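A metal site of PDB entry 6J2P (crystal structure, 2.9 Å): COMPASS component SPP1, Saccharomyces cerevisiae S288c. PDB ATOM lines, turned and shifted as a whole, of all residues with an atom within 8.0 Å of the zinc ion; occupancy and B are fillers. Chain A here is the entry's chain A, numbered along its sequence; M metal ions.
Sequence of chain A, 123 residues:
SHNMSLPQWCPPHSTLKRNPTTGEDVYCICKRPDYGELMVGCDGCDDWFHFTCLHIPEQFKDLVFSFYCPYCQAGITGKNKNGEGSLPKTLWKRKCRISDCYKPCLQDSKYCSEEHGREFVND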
ATOM      1  N   LYS A  95      -9.943  10.149  16.195  1.00  0.00           N
ATOM      2  CA  LYS A  95     -10.053  11.142  15.142  1.00  0.00           C
ATOM      3  C   LYS A  95     -11.448  11.753  15.105  1.00  0.00           C
ATOM      4  O   LYS A  95     -12.439  11.066  15.359  1.00  0.00           O
ATOM      5  CB  LYS A  95      -9.702  10.501  13.791  1.00  0.00           C
ATOM      6  CG  LYS A  95     -10.124  11.280  12.554  1.00  0.00           C
ATOM      7  CD  LYS A  95     -10.448  10.313  11.416  1.00  0.00           C
ATOM      8  CE  LYS A  95     -11.472  10.895  10.450  1.00  0.00           C
ATOM      9  NZ  LYS A  95     -12.863  10.474  10.782  1.00  0.00           N
ATOM     10  N   CYS A  96     -11.503  13.054  14.815  1.00  0.00           N
ATOM     11  CA  CYS A  96     -12.778  13.750  14.652  1.00  0.00           C
ATOM     12  C   CYS A  96     -13.661  13.011  13.654  1.00  0.00           C
ATOM     13  O   CYS A  96     -13.213  12.602  12.579  1.00  0.00           O
ATOM     14  CB  CYS A  96     -12.540  15.182  14.188  1.00  0.00           C
ATOM     15  SG  CYS A  96     -14.020  16.070  13.617  1.00  0.00           S
ATOM     16  N   ARG A  97     -14.930  12.833  14.028  1.00  0.00           N
ATOM     17  CA  ARG A  97     -15.838  11.983  13.263  1.00  0.00           C
ATOM     18  C   ARG A  97     -16.263  12.583  11.928  1.00  0.00           C
ATOM     19  O   ARG A  97     -16.910  11.900  11.139  1.00  0.00           O
ATOM     20  CB  ARG A  97     -17.069  11.656  14.113  1.00  0.00           C
ATOM     21  CG  ARG A  97     -16.733  11.172  15.531  1.00  0.00           C
ATOM     22  CD  ARG A  97     -17.389   9.840  15.841  1.00  0.00           C
ATOM     23  NE  ARG A  97     -18.799   9.834  15.485  1.00  0.00           N
ATOM     24  CZ  ARG A  97     -19.523   8.736  15.266  1.00  0.00           C
ATOM     25  NH1 ARG A  97     -18.960   7.542  15.378  1.00  0.00           N
ATOM     26  NH2 ARG A  97     -20.814   8.825  14.947  1.00  0.00           N
ATOM     27  N   ILE A  98     -15.910  13.839  11.651  1.00  0.00           N
ATOM     28  CA  ILE A  98     -16.054  14.378  10.300  1.00  0.00           C
ATOM     29  C   ILE A  98     -15.083  13.644   9.391  1.00  0.00           C
ATOM     30  O   ILE A  98     -13.875  13.619   9.639  1.00  0.00           O
ATOM     31  CB  ILE A  98     -15.811  15.891  10.283  1.00  0.00           C
ATOM     32  CG1 ILE A  98     -16.790  16.606  11.222  1.00  0.00           C
ATOM     33  CG2 ILE A  98     -15.949  16.440   8.858  1.00  0.00           C
ATOM     34  CD1 ILE A  98     -18.244  16.422  10.844  1.00  0.00           C
ATOM     35  N   SER A  99     -15.613  13.039   8.320  1.00  0.00           N
ATOM     36  CA  SER A  99     -14.780  12.193   7.457  1.00  0.00           C
ATOM     37  C   SER A  99     -13.646  12.983   6.814  1.00  0.00           C
ATOM     38  O   SER A  99     -12.604  12.412   6.478  1.00  0.00           O
ATOM     39  CB  SER A  99     -15.638  11.530   6.387  1.00  0.00           C
ATOM     40  OG  SER A  99     -16.391  12.481   5.657  1.00  0.00           O
ATOM     41  N   ASP A 100     -13.825  14.294   6.639  1.00  0.00           N
ATOM     42  CA  ASP A 100     -12.777  15.123   6.056  1.00  0.00           C
ATOM     43  C   ASP A 100     -11.641  15.374   7.045  1.00  0.00           C
ATOM     44  O   ASP A 100     -10.465  15.333   6.657  1.00  0.00           O
ATOM     45  CB  ASP A 100     -13.359  16.457   5.590  1.00  0.00           C
ATOM     46  CG  ASP A 100     -13.824  16.410   4.154  1.00  0.00           C
ATOM     47  OD1 ASP A 100     -13.526  17.358   3.393  1.00  0.00           O
ATOM     48  OD2 ASP A 100     -14.500  15.429   3.782  1.00  0.00           O
ATOM     49  N   CYS A 101     -11.966  15.608   8.310  1.00  0.00           N
ATOM     50  CA  CYS A 101     -10.968  16.019   9.290  1.00  0.00           C
ATOM     51  C   CYS A 101     -10.090  14.850   9.701  1.00  0.00           C
ATOM     52  O   CYS A 101     -10.550  13.707   9.776  1.00  0.00           O
ATOM     53  CB  CYS A 101     -11.652  16.617  10.511  1.00  0.00           C
ATOM     54  SG  CYS A 101     -10.657  17.845  11.393  1.00  0.00           S
ATOM     55  N   TYR A 102      -8.820  15.133   9.966  1.00  0.00           N
ATOM     56  CA  TYR A 102      -7.889  14.131  10.493  1.00  0.00           C
ATOM     57  C   TYR A 102      -7.168  14.661  11.728  1.00  0.00           C
ATOM     58  O   TYR A 102      -6.032  14.290  11.997  1.00  0.00           O
ATOM     59  CB  TYR A 102      -6.900  13.675   9.425  1.00  0.00           C
ATOM     60  CG  TYR A 102      -7.532  12.823   8.349  1.00  0.00           C
ATOM     61  CD1 TYR A 102      -7.747  11.474   8.544  1.00  0.00           C
ATOM     62  CD2 TYR A 102      -7.933  13.384   7.140  1.00  0.00           C
ATOM     63  CE1 TYR A 102      -8.329  10.687   7.557  1.00  0.00           C
ATOM     64  CE2 TYR A 102      -8.520  12.619   6.154  1.00  0.00           C
ATOM     65  CZ  TYR A 102      -8.720  11.268   6.368  1.00  0.00           C
ATOM     66  OH  TYR A 102      -9.311  10.507   5.390  1.00  0.00           O
ATOM     67  N   LYS A 103      -7.840  15.550  12.492  1.00  0.00           N
ATOM     68  CA  LYS A 103      -7.448  16.163  13.746  1.00  0.00           C
ATOM     69  C   LYS A 103      -8.015  15.376  14.917  1.00  0.00           C
ATOM     70  O   LYS A 103      -9.107  14.797  14.817  1.00  0.00           O
ATOM     71  CB  LYS A 103      -7.945  17.617  13.808  1.00  0.00           C
ATOM     72  CG  LYS A 103      -6.867  18.667  13.594  1.00  0.00           C
ATOM     73  CD  LYS A 103      -6.205  18.514  12.237  1.00  0.00           C
ATOM     74  CE  LYS A 103      -7.165  18.819  11.107  1.00  0.00           C
ATOM     75  NZ  LYS A 103      -6.650  18.328   9.789  1.00  0.00           N
ATOM     76  N   PRO A 104      -7.307  15.319  16.037  1.00  0.00           N
ATOM     77  CA  PRO A 104      -7.786  14.530  17.180  1.00  0.00           C
ATOM     78  C   PRO A 104      -8.994  15.169  17.849  1.00  0.00           C
ATOM     79  O   PRO A 104      -9.152  16.391  17.859  1.00  0.00           O
ATOM     80  CB  PRO A 104      -6.585  14.491  18.119  1.00  0.00           C
ATOM     81  CG  PRO A 104      -5.823  15.734  17.806  1.00  0.00           C
ATOM     82  CD  PRO A 104      -6.004  15.955  16.321  1.00  0.00           C
ATOM     83  N   CYS A 105      -9.842  14.310  18.410  1.00  0.00           N
ATOM     84  CA  CYS A 105     -11.018  14.788  19.135  1.00  0.00           C
ATOM     85  C   CYS A 105     -10.615  15.513  20.414  1.00  0.00           C
ATOM     86  O   CYS A 105      -9.508  15.341  20.936  1.00  0.00           O
ATOM     87  CB  CYS A 105     -11.943  13.619  19.492  1.00  0.00           C
ATOM     88  SG  CYS A 105     -12.910  12.926  18.129  1.00  0.00           S
ATOM     89  N   LYS A 110     -16.774  14.489  20.370  1.00  0.00           N
ATOM     90  CA  LYS A 110     -16.406  13.672  19.231  1.00  0.00           C
ATOM     91  C   LYS A 110     -15.920  14.499  18.050  1.00  0.00           C
ATOM     92  O   LYS A 110     -15.892  14.004  16.921  1.00  0.00           O
ATOM     93  CB  LYS A 110     -17.602  12.809  18.817  1.00  0.00           C
ATOM     94  CG  LYS A 110     -18.951  13.478  18.993  1.00  0.00           C
ATOM     95  CD  LYS A 110     -20.084  12.514  18.692  1.00  0.00           C
ATOM     96  CE  LYS A 110     -21.434  13.113  19.047  1.00  0.00           C
ATOM     97  NZ  LYS A 110     -22.549  12.128  18.933  1.00  0.00           N
ATOM     98  N   TYR A 111     -15.520  15.749  18.294  1.00  0.00           N
ATOM     99  CA  TYR A 111     -15.044  16.639  17.247  1.00  0.00           C
ATOM    100  C   TYR A 111     -13.759  17.329  17.691  1.00  0.00           C
ATOM    101  O   TYR A 111     -13.476  17.438  18.888  1.00  0.00           O
ATOM    102  CB  TYR A 111     -16.104  17.697  16.885  1.00  0.00           C
ATOM    103  CG  TYR A 111     -17.445  17.090  16.569  1.00  0.00           C
ATOM    104  CD1 TYR A 111     -17.710  16.574  15.307  1.00  0.00           C
ATOM    105  CD2 TYR A 111     -18.451  17.026  17.524  1.00  0.00           C
ATOM    106  CE1 TYR A 111     -18.927  16.022  15.013  1.00  0.00           C
ATOM    107  CE2 TYR A 111     -19.672  16.478  17.238  1.00  0.00           C
ATOM    108  CZ  TYR A 111     -19.907  15.963  15.978  1.00  0.00           C
ATOM    109  OH  TYR A 111     -21.133  15.410  15.680  1.00  0.00           O
ATOM    110  N   CYS A 112     -12.995  17.797  16.705  1.00  0.00           N
ATOM    111  CA  CYS A 112     -11.719  18.438  16.999  1.00  0.00           C
ATOM    112  C   CYS A 112     -11.891  19.838  17.570  1.00  0.00           C
ATOM    113  O   CYS A 112     -10.995  20.326  18.270  1.00  0.00           O
ATOM    114  CB  CYS A 112     -10.862  18.496  15.733  1.00  0.00           C
ATOM    115  SG  CYS A 112     -11.569  19.460  14.378  1.00  0.00           S
ATOM    116  N   SER A 113     -13.016  20.503  17.290  1.00  0.00           N
ATOM    117  CA  SER A 113     -13.273  21.841  17.801  1.00  0.00           C
ATOM    118  C   SER A 113     -14.770  22.118  17.692  1.00  0.00           C
ATOM    119  O   SER A 113     -15.558  21.255  17.294  1.00  0.00           O
ATOM    120  CB  SER A 113     -12.459  22.891  17.036  1.00  0.00           C
ATOM    121  OG  SER A 113     -12.587  24.174  17.637  1.00  0.00           O
ATOM    122  N   GLU A 114     -15.157  23.342  18.062  1.00  0.00           N
ATOM    123  CA  GLU A 114     -16.555  23.747  17.916  1.00  0.00           C
ATOM    124  C   GLU A 114     -16.915  23.997  16.452  1.00  0.00           C
ATOM    125  O   GLU A 114     -18.061  23.795  16.051  1.00  0.00           O
ATOM    126  CB  GLU A 114     -16.838  24.990  18.762  1.00  0.00           C
ATOM    127  CG  GLU A 114     -18.244  25.556  18.609  1.00  0.00           C
ATOM    128  CD  GLU A 114     -19.326  24.504  18.749  1.00  0.00           C
ATOM    129  OE1 GLU A 114     -19.284  23.730  19.727  1.00  0.00           O
ATOM    130  OE2 GLU A 114     -20.219  24.448  17.883  1.00  0.00           O
ATOM    131  N   GLU A 115     -15.937  24.418  15.641  1.00  0.00           N
ATOM    132  CA  GLU A 115     -16.168  24.694  14.227  1.00  0.00           C
ATOM    133  C   GLU A 115     -16.589  23.454  13.448  1.00  0.00           C
ATOM    134  O   GLU A 115     -17.042  23.591  12.305  1.00  0.00           O
ATOM    135  CB  GLU A 115     -14.918  25.306  13.602  1.00  0.00           C
ATOM    136  CG  GLU A 115     -14.331  26.482  14.383  1.00  0.00           C
ATOM    137  CD  GLU A 115     -13.097  26.111  15.182  1.00  0.00           C
ATOM    138  OE1 GLU A 115     -12.273  25.323  14.674  1.00  0.00           O
ATOM    139  OE2 GLU A 115     -12.954  26.602  16.324  1.00  0.00           O
ATOM    140  N   HIS A 116     -16.448  22.256  14.022  1.00  0.00           N
ATOM    141  CA  HIS A 116     -16.876  21.021  13.370  1.00  0.00           C
ATOM    142  C   HIS A 116     -17.969  20.295  14.125  1.00  0.00           C
ATOM    143  O   HIS A 116     -18.362  19.193  13.705  1.00  0.00           O
ATOM    144  CB  HIS A 116     -15.667  20.079  13.183  1.00  0.00           C
ATOM    145  CG  HIS A 116     -14.844  20.373  11.970  1.00  0.00           C
ATOM    146  ND1 HIS A 116     -14.263  19.375  11.213  1.00  0.00           N
ATOM    147  CD2 HIS A 116     -14.504  21.536  11.381  1.00  0.00           C
ATOM    148  CE1 HIS A 116     -13.597  19.924  10.215  1.00  0.00           C
ATOM    149  NE2 HIS A 116     -13.720  21.232  10.287  1.00  0.00           N
ATOM    150  N   GLY A 117     -18.495  20.871  15.204  1.00  0.00           N
ATOM    151  CA  GLY A 117     -19.481  20.199  16.021  1.00  0.00           C
ATOM    152  C   GLY A 117     -20.899  20.261  15.484  1.00  0.00           C
ATOM    153  O   GLY A 117     -21.761  20.938  16.062  1.00  0.00           O
HETATM  154 ZN    ZN M   1     -12.658  18.063  12.818  1.00  0.00          ZN
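SG of Cys 105 lies close to N of Cys 96, 3.6 Å away.
The backbone NH of Cys 96 sits at hydrogen-bond distance from the backbone carbonyl oxygen of Lys 103.
The backbone NH (N) of Lys 103 sits close to the side-chain sulfur (SG) of Cys 101 (3.8 Å).
SG of Cys 96 lies close to N of Ile 98.
Four residues have an atom within 4 Å of the zinc ion: Cys 96, Cys 101, Cys 112 and His 116.
The nearest printed residue that does not touch the zinc ion is Ile 98 (4.6 Å).
The side-chain sulfur (SG) of Cys 112 is bound to the zinc ion.
The zinc ion is bound by the side-chain sulfur (SG) of Cys 101, 2.5 Å away.
The zinc ion is bound by SG of Cys 96 (2.5 Å).
The zinc ion has three donor atoms within binding distance.
Slightly farther from the zinc ion lies a ring nitrogen (ND1) of His 116 (2.6 Å).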
